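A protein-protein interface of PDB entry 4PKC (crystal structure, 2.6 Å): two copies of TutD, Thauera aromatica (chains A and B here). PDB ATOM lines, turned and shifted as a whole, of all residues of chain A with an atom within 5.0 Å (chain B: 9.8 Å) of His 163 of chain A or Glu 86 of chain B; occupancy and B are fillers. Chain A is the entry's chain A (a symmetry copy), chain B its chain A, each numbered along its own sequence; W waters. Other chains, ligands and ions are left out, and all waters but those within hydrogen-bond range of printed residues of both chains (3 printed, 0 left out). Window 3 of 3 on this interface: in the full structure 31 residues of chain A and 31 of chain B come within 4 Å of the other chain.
Of chain B, only Glu 86 and Gly 87 come within 4 Å of His 163 of chain A. Of chain A, only Glu 86 (3.4 Å), Pro 162 (3.2 Å) and His 163 (3.0 Å) come within 4 Å of Glu 86 of chain B. Pro 162 of chain A touches just these residues of chain B: Glu 86 and Gly 87. No residue of chain B comes within 4 Å of Ser 164 of chain A. Printed residues of chain A within 4 Å of His 163 of chain B: Glu 86. Of the printed residues of chain A, Gly 87 of chain B touches Pro 162 (3.3 Å), His 163 (3.9 Å) and Lys 168 (2.7 Å). Lys 161 of chain A touches none of the printed residues of chain B. Arg 93 of chain B touches none of the printed residues of chain A. The nearest residue of chain B that does not touch His 163 of chain A is Lys 88 of chain B (6.5 Å). The nearest printed residue of chain A that does not touch Glu 86 of chain B is His 82 of chain A (5.7 Å). The nearest printed residue of chain A that does not touch His 163 of chain B is His 82 of chain A (7.8 Å).
NE2 of His 163 of chain A lies within hydrogen-bond range of OE2 of Glu 86 of chain B (3.0 Å). A ring nitrogen (NE2) of His 163 of chain B sits at hydrogen-bond distance from the side-chain carboxylate of Glu 86 of chain A (3.0 Å). The side-chain carboxylate (OE1) of Glu 86 of chain A lies close to the side-chain carboxylate (OE1) of Glu 86 of chain B (3.4 Å). The backbone carbonyl oxygen (O) of Gly 87 of chain B is in hydrogen-bond range of the side-chain amino group (NZ) of Lys 168 of chain A.
ND1 of His 163 of chain A lies within hydrogen-bond range of O of Tyr 159 of chain A (3.4 Å). ND1 of His 163 of chain B sits at hydrogen-bond distance from O of Tyr 159 of chain B, 3.4 Å away. OE1 of Glu 86 of chain B is in salt-bridge range of NH2 of Arg 93 of chain B.
Of the 23 printed residues of chain B, 4 touch a printed residue of chain A. Hydrophobic or aromatic side chains of chain B that line the printed part of chain A: Pro 162 and His 163. Hydrophobic or aromatic side chains of chain A within 4 Å of the printed part of chain B: Pro 162 and His 163. Among the printed residues, 8 pairs touch across the chains. Among the printed residues, no Asp or Glu carboxylate lies within 4 Å of a Lys or Arg side-chain nitrogen of the other chain.
Glu 86 of chain B touches its own counterpart, Glu 86 of chain A. Glu 86 of chain A touches Pro 162 of chain B, and with the chains exchanged Pro 162 of chain A touches Glu 86 of chain B. Glu 86 of chain A touches His 163 of chain B, and with the chains exchanged His 163 of chain A touches Glu 86 of chain B. 6 positions are printed for both chains.
Water W2 lies within hydrogen-bond range of the side-chain carboxylate of Glu 86 of chain B, a ring nitrogen (NE2) of His 163 of chain B, the side-chain carboxylate of Glu 86 of chain A and the guanidinium group of Arg 93 of chain B. Water W1 lies within hydrogen-bond range of OE1 of Glu 86 of chain A (2.7 Å), NE2 of His 163 of chain A (2.9 Å) and OE2 of Glu 86 of chain B (3.1 Å). Water W3 lies within hydrogen-bond range of O of Lys 88 of chain B (2.8 Å), O of Gly 87 of chain B (3.2 Å) and NZ of Lys 168 of chain A (3.5 Å).
Among the printed residues, pairs that only touch across the chains: Glu 86 of chain A with Pro 162 of chain B (3.2 Å), Pro 162 of chain A with Glu 86 of chain B (3.2 Å), Pro 162 of chain A with Gly 87 of chain B (3.3 Å) and His 163 of chain A with Gly 87 of chain B (3.9 Å).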
ATOM      1  N   HIS A  82      -7.452  -4.094 -16.823  1.00  0.00           N
ATOM      2  CA  HIS A  82      -6.159  -3.943 -17.482  1.00  0.00           C
ATOM      3  C   HIS A  82      -6.323  -3.412 -18.902  1.00  0.00           C
ATOM      4  O   HIS A  82      -5.550  -2.566 -19.350  1.00  0.00           O
ATOM      5  CB  HIS A  82      -5.403  -5.272 -17.502  1.00  0.00           C
ATOM      6  CG  HIS A  82      -3.966  -5.143 -17.905  1.00  0.00           C
ATOM      7  ND1 HIS A  82      -3.530  -5.362 -19.195  1.00  0.00           N
ATOM      8  CD2 HIS A  82      -2.866  -4.816 -17.188  1.00  0.00           C
ATOM      9  CE1 HIS A  82      -2.224  -5.176 -19.254  1.00  0.00           C
ATOM     10  NE2 HIS A  82      -1.796  -4.843 -18.048  1.00  0.00           N
ATOM     11  N   GLU A  86      -5.114   0.983 -20.129  1.00  0.00           N
ATOM     12  CA  GLU A  86      -3.993   1.138 -21.054  1.00  0.00           C
ATOM     13  C   GLU A  86      -3.518   2.585 -21.134  1.00  0.00           C
ATOM     14  O   GLU A  86      -4.326   3.509 -21.211  1.00  0.00           O
ATOM     15  CB  GLU A  86      -4.380   0.641 -22.447  1.00  0.00           C
ATOM     16  CG  GLU A  86      -4.290  -0.865 -22.618  1.00  0.00           C
ATOM     17  CD  GLU A  86      -2.859  -1.365 -22.600  1.00  0.00           C
ATOM     18  OE1 GLU A  86      -2.658  -2.598 -22.628  1.00  0.00           O
ATOM     19  OE2 GLU A  86      -1.932  -0.524 -22.562  1.00  0.00           O
ATOM     20  N   GLU A 131      -1.564 -12.826 -13.953  1.00  0.00           N
ATOM     21  CA  GLU A 131      -0.581 -11.751 -14.021  1.00  0.00           C
ATOM     22  C   GLU A 131       0.770 -12.196 -13.467  1.00  0.00           C
ATOM     23  O   GLU A 131       1.767 -11.490 -13.603  1.00  0.00           O
ATOM     24  CB  GLU A 131      -1.071 -10.515 -13.261  1.00  0.00           C
ATOM     25  CG  GLU A 131      -0.939 -10.609 -11.744  1.00  0.00           C
ATOM     26  CD  GLU A 131      -2.077 -11.375 -11.092  1.00  0.00           C
ATOM     27  OE1 GLU A 131      -2.905 -11.964 -11.820  1.00  0.00           O
ATOM     28  OE2 GLU A 131      -2.146 -11.381  -9.845  1.00  0.00           O
ATOM     29  N   TYR A 159      -4.347 -13.656 -22.962  1.00  0.00           N
ATOM     30  CA  TYR A 159      -4.215 -12.205 -22.952  1.00  0.00           C
ATOM     31  C   TYR A 159      -3.116 -11.756 -21.991  1.00  0.00           C
ATOM     32  O   TYR A 159      -2.343 -10.850 -22.297  1.00  0.00           O
ATOM     33  CB  TYR A 159      -5.549 -11.551 -22.572  1.00  0.00           C
ATOM     34  CG  TYR A 159      -5.447 -10.089 -22.195  1.00  0.00           C
ATOM     35  CD1 TYR A 159      -5.529  -9.095 -23.161  1.00  0.00           C
ATOM     36  CD2 TYR A 159      -5.277  -9.701 -20.870  1.00  0.00           C
ATOM     37  CE1 TYR A 159      -5.438  -7.757 -22.819  1.00  0.00           C
ATOM     38  CE2 TYR A 159      -5.182  -8.370 -20.521  1.00  0.00           C
ATOM     39  CZ  TYR A 159      -5.263  -7.401 -21.498  1.00  0.00           C
ATOM     40  OH  TYR A 159      -5.171  -6.073 -21.151  1.00  0.00           O
ATOM     41  N   TRP A 160      -3.058 -12.395 -20.827  1.00  0.00           N
ATOM     42  CA  TRP A 160      -2.112 -12.008 -19.784  1.00  0.00           C
ATOM     43  C   TRP A 160      -0.699 -12.519 -20.032  1.00  0.00           C
ATOM     44  O   TRP A 160       0.248 -12.040 -19.409  1.00  0.00           O
ATOM     45  CB  TRP A 160      -2.595 -12.506 -18.417  1.00  0.00           C
ATOM     46  CG  TRP A 160      -3.562 -11.583 -17.749  1.00  0.00           C
ATOM     47  CD1 TRP A 160      -4.912 -11.745 -17.646  1.00  0.00           C
ATOM     48  CD2 TRP A 160      -3.254 -10.346 -17.096  1.00  0.00           C
ATOM     49  NE1 TRP A 160      -5.464 -10.686 -16.965  1.00  0.00           N
ATOM     50  CE2 TRP A 160      -4.467  -9.814 -16.617  1.00  0.00           C
ATOM     51  CE3 TRP A 160      -2.069  -9.637 -16.870  1.00  0.00           C
ATOM     52  CZ2 TRP A 160      -4.530  -8.606 -15.925  1.00  0.00           C
ATOM     53  CZ3 TRP A 160      -2.135  -8.438 -16.183  1.00  0.00           C
ATOM     54  CH2 TRP A 160      -3.356  -7.935 -15.719  1.00  0.00           C
ATOM     55  N   LYS A 161      -0.560 -13.485 -20.936  1.00  0.00           N
ATOM     56  CA  LYS A 161       0.724 -14.151 -21.153  1.00  0.00           C
ATOM     57  C   LYS A 161       1.891 -13.190 -21.422  1.00  0.00           C
ATOM     58  O   LYS A 161       2.933 -13.310 -20.780  1.00  0.00           O
ATOM     59  CB  LYS A 161       0.618 -15.164 -22.297  1.00  0.00           C
ATOM     60  CG  LYS A 161       1.888 -15.974 -22.507  1.00  0.00           C
ATOM     61  CD  LYS A 161       1.704 -17.051 -23.560  1.00  0.00           C
ATOM     62  CE  LYS A 161       2.962 -17.892 -23.711  1.00  0.00           C
ATOM     63  NZ  LYS A 161       2.811 -18.937 -24.760  1.00  0.00           N
ATOM     64  N   PRO A 162       1.732 -12.232 -22.357  1.00  0.00           N
ATOM     65  CA  PRO A 162       2.890 -11.358 -22.570  1.00  0.00           C
ATOM     66  C   PRO A 162       3.078 -10.330 -21.453  1.00  0.00           C
ATOM     67  O   PRO A 162       4.149  -9.729 -21.352  1.00  0.00           O
ATOM     68  CB  PRO A 162       2.560 -10.666 -23.894  1.00  0.00           C
ATOM     69  CG  PRO A 162       1.080 -10.611 -23.912  1.00  0.00           C
ATOM     70  CD  PRO A 162       0.620 -11.891 -23.266  1.00  0.00           C
ATOM     71  N   HIS A 163       2.052 -10.138 -20.630  1.00  0.00           N
ATOM     72  CA  HIS A 163       2.122  -9.178 -19.533  1.00  0.00           C
ATOM     73  C   HIS A 163       2.515  -9.844 -18.222  1.00  0.00           C
ATOM     74  O   HIS A 163       2.768  -9.165 -17.227  1.00  0.00           O
ATOM     75  CB  HIS A 163       0.785  -8.455 -19.363  1.00  0.00           C
ATOM     76  CG  HIS A 163       0.388  -7.628 -20.545  1.00  0.00           C
ATOM     77  ND1 HIS A 163      -0.460  -8.091 -21.527  1.00  0.00           N
ATOM     78  CD2 HIS A 163       0.725  -6.366 -20.903  1.00  0.00           C
ATOM     79  CE1 HIS A 163      -0.631  -7.150 -22.439  1.00  0.00           C
ATOM     80  NE2 HIS A 163       0.079  -6.094 -22.083  1.00  0.00           N
ATOM     81  N   SER A 164       2.568 -11.172 -18.226  1.00  0.00           N
ATOM     82  CA  SER A 164       2.863 -11.931 -17.016  1.00  0.00           C
ATOM     83  C   SER A 164       4.276 -11.659 -16.524  1.00  0.00           C
ATOM     84  O   SER A 164       5.167 -11.345 -17.312  1.00  0.00           O
ATOM     85  CB  SER A 164       2.684 -13.430 -17.262  1.00  0.00           C
ATOM     86  OG  SER A 164       3.746 -13.945 -18.047  1.00  0.00           O
ATOM     87  N   LEU A 165       4.468 -11.783 -15.215  1.00  0.00           N
ATOM     88  CA  LEU A 165       5.778 -11.611 -14.600  1.00  0.00           C
ATOM     89  C   LEU A 165       6.774 -12.616 -15.165  1.00  0.00           C
ATOM     90  O   LEU A 165       7.959 -12.320 -15.315  1.00  0.00           O
ATOM     91  CB  LEU A 165       5.678 -11.761 -13.083  1.00  0.00           C
ATOM     92  CG  LEU A 165       6.980 -11.649 -12.288  1.00  0.00           C
ATOM     93  CD1 LEU A 165       7.597 -10.267 -12.461  1.00  0.00           C
ATOM     94  CD2 LEU A 165       6.737 -11.960 -10.818  1.00  0.00           C
ATOM     95  N   LYS A 168       8.271 -11.521 -18.527  1.00  0.00           N
ATOM     96  CA  LYS A 168       9.118 -10.337 -18.454  1.00  0.00           C
ATOM     97  C   LYS A 168      10.516 -10.654 -17.932  1.00  0.00           C
ATOM     98  O   LYS A 168      11.468  -9.926 -18.209  1.00  0.00           O
ATOM     99  CB  LYS A 168       8.464  -9.267 -17.576  1.00  0.00           C
ATOM    100  CG  LYS A 168       7.230  -8.633 -18.198  1.00  0.00           C
ATOM    101  CD  LYS A 168       6.729  -7.464 -17.369  1.00  0.00           C
ATOM    102  CE  LYS A 168       5.530  -6.799 -18.024  1.00  0.00           C
ATOM    103  NZ  LYS A 168       5.861  -6.242 -19.363  1.00  0.00           N
ATOM    104  N   LEU B  78       1.938   0.946 -37.649  1.00  0.00           N
ATOM    105  CA  LEU B  78       2.427   1.281 -36.318  1.00  0.00           C
ATOM    106  C   LEU B  78       1.447   0.761 -35.272  1.00  0.00           C
ATOM    107  O   LEU B  78       1.844   0.316 -34.194  1.00  0.00           O
ATOM    108  CB  LEU B  78       2.621   2.792 -36.169  1.00  0.00           C
ATOM    109  CG  LEU B  78       3.476   3.281 -34.997  1.00  0.00           C
ATOM    110  CD1 LEU B  78       4.936   2.897 -35.200  1.00  0.00           C
ATOM    111  CD2 LEU B  78       3.333   4.784 -34.808  1.00  0.00           C
ATOM    112  N   THR B  79       0.162   0.817 -35.610  1.00  0.00           N
ATOM    113  CA  THR B  79      -0.897   0.343 -34.727  1.00  0.00           C
ATOM    114  C   THR B  79      -0.877  -1.177 -34.617  1.00  0.00           C
ATOM    115  O   THR B  79      -1.004  -1.733 -33.523  1.00  0.00           O
ATOM    116  CB  THR B  79      -2.279   0.800 -35.223  1.00  0.00           C
ATOM    117  OG1 THR B  79      -2.316   2.231 -35.271  1.00  0.00           O
ATOM    118  CG2 THR B  79      -3.379   0.298 -34.300  1.00  0.00           C
ATOM    119  N   GLU B  80      -0.719  -1.840 -35.758  1.00  0.00           N
ATOM    120  CA  GLU B  80      -0.636  -3.296 -35.805  1.00  0.00           C
ATOM    121  C   GLU B  80       0.520  -3.810 -34.954  1.00  0.00           C
ATOM    122  O   GLU B  80       0.358  -4.743 -34.167  1.00  0.00           O
ATOM    123  CB  GLU B  80      -0.476  -3.774 -37.249  1.00  0.00           C
ATOM    124  CG  GLU B  80      -0.272  -5.274 -37.393  1.00  0.00           C
ATOM    125  CD  GLU B  80      -0.098  -5.701 -38.839  1.00  0.00           C
ATOM    126  OE1 GLU B  80       0.547  -4.958 -39.607  1.00  0.00           O
ATOM    127  OE2 GLU B  80      -0.614  -6.777 -39.209  1.00  0.00           O
ATOM    128  N   ALA B  81       1.685  -3.188 -35.113  1.00  0.00           N
ATOM    129  CA  ALA B  81       2.878  -3.593 -34.382  1.00  0.00           C
ATOM    130  C   ALA B  81       2.729  -3.349 -32.884  1.00  0.00           C
ATOM    131  O   ALA B  81       3.201  -4.144 -32.073  1.00  0.00           O
ATOM    132  CB  ALA B  81       4.099  -2.861 -34.915  1.00  0.00           C
ATOM    133  N   HIS B  82       2.075  -2.250 -32.522  1.00  0.00           N
ATOM    134  CA  HIS B  82       1.912  -1.891 -31.117  1.00  0.00           C
ATOM    135  C   HIS B  82       1.025  -2.897 -30.390  1.00  0.00           C
ATOM    136  O   HIS B  82       1.301  -3.269 -29.250  1.00  0.00           O
ATOM    137  CB  HIS B  82       1.330  -0.483 -30.981  1.00  0.00           C
ATOM    138  CG  HIS B  82       1.393   0.065 -29.589  1.00  0.00           C
ATOM    139  ND1 HIS B  82       0.330   0.000 -28.712  1.00  0.00           N
ATOM    140  CD2 HIS B  82       2.392   0.686 -28.920  1.00  0.00           C
ATOM    141  CE1 HIS B  82       0.672   0.558 -27.566  1.00  0.00           C
ATOM    142  NE2 HIS B  82       1.920   0.983 -27.665  1.00  0.00           N
ATOM    143  N   LYS B  83      -0.040  -3.332 -31.056  1.00  0.00           N
ATOM    144  CA  LYS B  83      -0.933  -4.336 -30.495  1.00  0.00           C
ATOM    145  C   LYS B  83      -0.207  -5.662 -30.314  1.00  0.00           C
ATOM    146  O   LYS B  83      -0.455  -6.392 -29.355  1.00  0.00           O
ATOM    147  CB  LYS B  83      -2.160  -4.534 -31.388  1.00  0.00           C
ATOM    148  CG  LYS B  83      -3.127  -3.364 -31.409  1.00  0.00           C
ATOM    149  CD  LYS B  83      -4.250  -3.600 -32.410  1.00  0.00           C
ATOM    150  CE  LYS B  83      -5.195  -2.409 -32.473  1.00  0.00           C
ATOM    151  NZ  LYS B  83      -6.209  -2.546 -33.558  1.00  0.00           N
ATOM    152  N   ALA B  84       0.695  -5.964 -31.241  1.00  0.00           N
ATOM    153  CA  ALA B  84       1.384  -7.248 -31.245  1.00  0.00           C
ATOM    154  C   ALA B  84       2.601  -7.254 -30.327  1.00  0.00           C
ATOM    155  O   ALA B  84       3.116  -8.317 -29.981  1.00  0.00           O
ATOM    156  CB  ALA B  84       1.794  -7.617 -32.662  1.00  0.00           C
ATOM    157  N   SER B  85       3.058  -6.070 -29.932  1.00  0.00           N
ATOM    158  CA  SER B  85       4.267  -5.954 -29.122  1.00  0.00           C
ATOM    159  C   SER B  85       3.968  -5.730 -27.643  1.00  0.00           C
ATOM    160  O   SER B  85       4.851  -5.337 -26.883  1.00  0.00           O
ATOM    161  CB  SER B  85       5.148  -4.817 -29.640  1.00  0.00           C
ATOM    162  OG  SER B  85       4.490  -3.568 -29.507  1.00  0.00           O
ATOM    163  N   GLU B  86       2.724  -5.978 -27.243  1.00  0.00           N
ATOM    164  CA  GLU B  86       2.312  -5.813 -25.851  1.00  0.00           C
ATOM    165  C   GLU B  86       3.149  -6.668 -24.905  1.00  0.00           C
ATOM    166  O   GLU B  86       3.418  -7.835 -25.184  1.00  0.00           O
ATOM    167  CB  GLU B  86       0.831  -6.160 -25.691  1.00  0.00           C
ATOM    168  CG  GLU B  86      -0.116  -5.041 -26.085  1.00  0.00           C
ATOM    169  CD  GLU B  86      -0.062  -3.870 -25.123  1.00  0.00           C
ATOM    170  OE1 GLU B  86      -0.720  -2.843 -25.397  1.00  0.00           O
ATOM    171  OE2 GLU B  86       0.635  -3.978 -24.090  1.00  0.00           O
ATOM    172  N   GLY B  87       3.562  -6.075 -23.789  1.00  0.00           N
ATOM    173  CA  GLY B  87       4.346  -6.783 -22.791  1.00  0.00           C
ATOM    174  C   GLY B  87       5.841  -6.578 -22.938  1.00  0.00           C
ATOM    175  O   GLY B  87       6.574  -6.576 -21.949  1.00  0.00           O
ATOM    176  N   LYS B  88       6.293  -6.408 -24.175  1.00  0.00           N
ATOM    177  CA  LYS B  88       7.715  -6.241 -24.469  1.00  0.00           C
ATOM    178  C   LYS B  88       8.236  -4.901 -23.950  1.00  0.00           C
ATOM    179  O   LYS B  88       7.450  -3.983 -23.709  1.00  0.00           O
ATOM    180  CB  LYS B  88       7.953  -6.357 -25.978  1.00  0.00           C
ATOM    181  CG  LYS B  88       7.482  -7.672 -26.577  1.00  0.00           C
ATOM    182  CD  LYS B  88       7.689  -7.693 -28.082  1.00  0.00           C
ATOM    183  CE  LYS B  88       7.129  -8.961 -28.708  1.00  0.00           C
ATOM    184  NZ  LYS B  88       7.839 -10.182 -28.234  1.00  0.00           N
ATOM    185  N   PRO B  89       9.563  -4.787 -23.758  1.00  0.00           N
ATOM    186  CA  PRO B  89      10.141  -3.497 -23.358  1.00  0.00           C
ATOM    187  C   PRO B  89       9.818  -2.406 -24.374  1.00  0.00           C
ATOM    188  O   PRO B  89       9.895  -2.661 -25.576  1.00  0.00           O
ATOM    189  CB  PRO B  89      11.645  -3.782 -23.314  1.00  0.00           C
ATOM    190  CG  PRO B  89      11.745  -5.248 -23.077  1.00  0.00           C
ATOM    191  CD  PRO B  89      10.580  -5.853 -23.806  1.00  0.00           C
ATOM    192  N   GLU B  90       9.462  -1.218 -23.893  1.00  0.00           N
ATOM    193  CA  GLU B  90       9.004  -0.129 -24.754  1.00  0.00           C
ATOM    194  C   GLU B  90       9.993   0.218 -25.865  1.00  0.00           C
ATOM    195  O   GLU B  90       9.588   0.537 -26.985  1.00  0.00           O
ATOM    196  CB  GLU B  90       8.713   1.118 -23.917  1.00  0.00           C
ATOM    197  CG  GLU B  90       7.568   0.948 -22.935  1.00  0.00           C
ATOM    198  CD  GLU B  90       6.254   0.624 -23.623  1.00  0.00           C
ATOM    199  OE1 GLU B  90       5.336   0.114 -22.945  1.00  0.00           O
ATOM    200  OE2 GLU B  90       6.136   0.881 -24.841  1.00  0.00           O
ATOM    201  N   ILE B  92      12.035  -1.812 -27.369  1.00  0.00           N
ATOM    202  CA  ILE B  92      11.916  -2.856 -28.377  1.00  0.00           C
ATOM    203  C   ILE B  92      10.602  -2.720 -29.146  1.00  0.00           C
ATOM    204  O   ILE B  92      10.560  -2.928 -30.360  1.00  0.00           O
ATOM    205  CB  ILE B  92      12.015  -4.259 -27.741  1.00  0.00           C
ATOM    206  CG1 ILE B  92      13.395  -4.451 -27.112  1.00  0.00           C
ATOM    207  CG2 ILE B  92      11.749  -5.346 -28.770  1.00  0.00           C
ATOM    208  CD1 ILE B  92      13.645  -5.851 -26.596  1.00  0.00           C
ATOM    209  N   ARG B  93       9.536  -2.356 -28.438  1.00  0.00           N
ATOM    210  CA  ARG B  93       8.237  -2.138 -29.070  1.00  0.00           C
ATOM    211  C   ARG B  93       8.314  -1.031 -30.114  1.00  0.00           C
ATOM    212  O   ARG B  93       7.688  -1.114 -31.170  1.00  0.00           O
ATOM    213  CB  ARG B  93       7.176  -1.784 -28.029  1.00  0.00           C
ATOM    214  CG  ARG B  93       6.979  -2.820 -26.939  1.00  0.00           C
ATOM    215  CD  ARG B  93       5.821  -2.423 -26.045  1.00  0.00           C
ATOM    216  NE  ARG B  93       4.546  -2.501 -26.753  1.00  0.00           N
ATOM    217  CZ  ARG B  93       3.416  -1.953 -26.317  1.00  0.00           C
ATOM    218  NH1 ARG B  93       3.403  -1.275 -25.177  1.00  0.00           N
ATOM    219  NH2 ARG B  93       2.302  -2.078 -27.025  1.00  0.00           N
ATOM    220  N   ARG B  94       9.084   0.007 -29.805  1.00  0.00           N
ATOM    221  CA  ARG B  94       9.277   1.131 -30.715  1.00  0.00           C
ATOM    222  C   ARG B  94      10.105   0.721 -31.927  1.00  0.00           C
ATOM    223  O   ARG B  94       9.884   1.207 -33.037  1.00  0.00           O
ATOM    224  CB  ARG B  94       9.946   2.294 -29.986  1.00  0.00           C
ATOM    225  CG  ARG B  94       9.021   3.046 -29.044  1.00  0.00           C
ATOM    226  CD  ARG B  94       8.217   4.093 -29.795  1.00  0.00           C
ATOM    227  NE  ARG B  94       9.080   5.117 -30.379  1.00  0.00           N
ATOM    228  CZ  ARG B  94       8.641   6.149 -31.091  1.00  0.00           C
ATOM    229  NH1 ARG B  94       9.500   7.032 -31.583  1.00  0.00           N
ATOM    230  NH2 ARG B  94       7.342   6.300 -31.312  1.00  0.00           N
ATOM    231  N   LEU B  96      10.179  -2.399 -33.080  1.00  0.00           N
ATOM    232  CA  LEU B  96       9.286  -3.280 -33.822  1.00  0.00           C
ATOM    233  C   LEU B  96       8.238  -2.469 -34.576  1.00  0.00           C
ATOM    234  O   LEU B  96       7.774  -2.875 -35.641  1.00  0.00           O
ATOM    235  CB  LEU B  96       8.608  -4.276 -32.880  1.00  0.00           C
ATOM    236  CG  LEU B  96       9.520  -5.323 -32.240  1.00  0.00           C
ATOM    237  CD1 LEU B  96       8.781  -6.076 -31.151  1.00  0.00           C
ATOM    238  CD2 LEU B  96      10.056  -6.283 -33.290  1.00  0.00           C
ATOM    239  N   GLY B  97       7.872  -1.322 -34.013  1.00  0.00           N
ATOM    240  CA  GLY B  97       6.952  -0.412 -34.664  1.00  0.00           C
ATOM    241  C   GLY B  97       7.560   0.145 -35.936  1.00  0.00           C
ATOM    242  O   GLY B  97       6.944   0.095 -36.999  1.00  0.00           O
ATOM    243  N   TYR B 159      -7.452   4.412 -30.620  1.00  0.00           N
ATOM    244  CA  TYR B 159      -6.616   3.398 -29.991  1.00  0.00           C
ATOM    245  C   TYR B 159      -5.352   4.015 -29.394  1.00  0.00           C
ATOM    246  O   TYR B 159      -4.930   3.650 -28.298  1.00  0.00           O
ATOM    247  CB  TYR B 159      -6.243   2.310 -31.006  1.00  0.00           C
ATOM    248  CG  TYR B 159      -5.111   1.405 -30.568  1.00  0.00           C
ATOM    249  CD1 TYR B 159      -5.360   0.262 -29.821  1.00  0.00           C
ATOM    250  CD2 TYR B 159      -3.793   1.689 -30.911  1.00  0.00           C
ATOM    251  CE1 TYR B 159      -4.327  -0.569 -29.421  1.00  0.00           C
ATOM    252  CE2 TYR B 159      -2.758   0.868 -30.514  1.00  0.00           C
ATOM    253  CZ  TYR B 159      -3.029  -0.259 -29.770  1.00  0.00           C
ATOM    254  OH  TYR B 159      -1.998  -1.080 -29.376  1.00  0.00           O
ATOM    255  N   TRP B 160      -4.755   4.951 -30.124  1.00  0.00           N
ATOM    256  CA  TRP B 160      -3.494   5.561 -29.711  1.00  0.00           C
ATOM    257  C   TRP B 160      -3.664   6.632 -28.643  1.00  0.00           C
ATOM    258  O   TRP B 160      -2.691   7.021 -27.999  1.00  0.00           O
ATOM    259  CB  TRP B 160      -2.774   6.165 -30.922  1.00  0.00           C
ATOM    260  CG  TRP B 160      -1.940   5.183 -31.678  1.00  0.00           C
ATOM    261  CD1 TRP B 160      -2.244   4.598 -32.872  1.00  0.00           C
ATOM    262  CD2 TRP B 160      -0.665   4.660 -31.286  1.00  0.00           C
ATOM    263  NE1 TRP B 160      -1.234   3.745 -33.251  1.00  0.00           N
ATOM    264  CE2 TRP B 160      -0.254   3.765 -32.294  1.00  0.00           C
ATOM    265  CE3 TRP B 160       0.168   4.863 -30.181  1.00  0.00           C
ATOM    266  CZ2 TRP B 160       0.955   3.075 -32.230  1.00  0.00           C
ATOM    267  CZ3 TRP B 160       1.366   4.175 -30.119  1.00  0.00           C
ATOM    268  CH2 TRP B 160       1.748   3.293 -31.137  1.00  0.00           C
ATOM    269  N   PRO B 162      -4.844   6.911 -25.492  1.00  0.00           N
ATOM    270  CA  PRO B 162      -4.278   6.815 -24.142  1.00  0.00           C
ATOM    271  C   PRO B 162      -2.772   6.553 -24.140  1.00  0.00           C
ATOM    272  O   PRO B 162      -2.123   6.727 -23.107  1.00  0.00           O
ATOM    273  CB  PRO B 162      -5.036   5.632 -23.536  1.00  0.00           C
ATOM    274  CG  PRO B 162      -5.346   4.769 -24.699  1.00  0.00           C
ATOM    275  CD  PRO B 162      -5.632   5.711 -25.837  1.00  0.00           C
ATOM    276  N   HIS B 163      -2.229   6.142 -25.283  1.00  0.00           N
ATOM    277  CA  HIS B 163      -0.802   5.858 -25.391  1.00  0.00           C
ATOM    278  C   HIS B 163      -0.027   7.052 -25.931  1.00  0.00           C
ATOM    279  O   HIS B 163       1.204   7.042 -25.948  1.00  0.00           O
ATOM    280  CB  HIS B 163      -0.561   4.640 -26.285  1.00  0.00           C
ATOM    281  CG  HIS B 163      -1.144   3.371 -25.750  1.00  0.00           C
ATOM    282  ND1 HIS B 163      -2.376   2.894 -26.140  1.00  0.00           N
ATOM    283  CD2 HIS B 163      -0.663   2.478 -24.851  1.00  0.00           C
ATOM    284  CE1 HIS B 163      -2.629   1.762 -25.509  1.00  0.00           C
ATOM    285  NE2 HIS B 163      -1.605   1.488 -24.719  1.00  0.00           N
ATOM    286  N   PHE B 582       8.523   5.987 -23.479  1.00  0.00           N
ATOM    287  CA  PHE B 582       7.503   5.412 -24.351  1.00  0.00           C
ATOM    288  C   PHE B 582       7.694   5.772 -25.823  1.00  0.00           C
ATOM    289  O   PHE B 582       7.130   5.122 -26.701  1.00  0.00           O
ATOM    290  CB  PHE B 582       6.112   5.851 -23.889  1.00  0.00           C
ATOM    291  CG  PHE B 582       5.722   5.308 -22.543  1.00  0.00           C
ATOM    292  CD1 PHE B 582       5.164   4.046 -22.427  1.00  0.00           C
ATOM    293  CD2 PHE B 582       5.913   6.059 -21.395  1.00  0.00           C
ATOM    294  CE1 PHE B 582       4.804   3.542 -21.190  1.00  0.00           C
ATOM    295  CE2 PHE B 582       5.555   5.560 -20.156  1.00  0.00           C
ATOM    296  CZ  PHE B 582       5.000   4.301 -20.054  1.00  0.00           C
HETATM  297  O   HOH W   1      -0.479  -3.382 -21.279  1.00  0.00           O
HETATM  298  O   HOH W   2       0.414  -0.564 -24.559  1.00  0.00           O
HETATM  299  O   HOH W   3       5.839  -3.469 -21.429  1.00  0.00           O
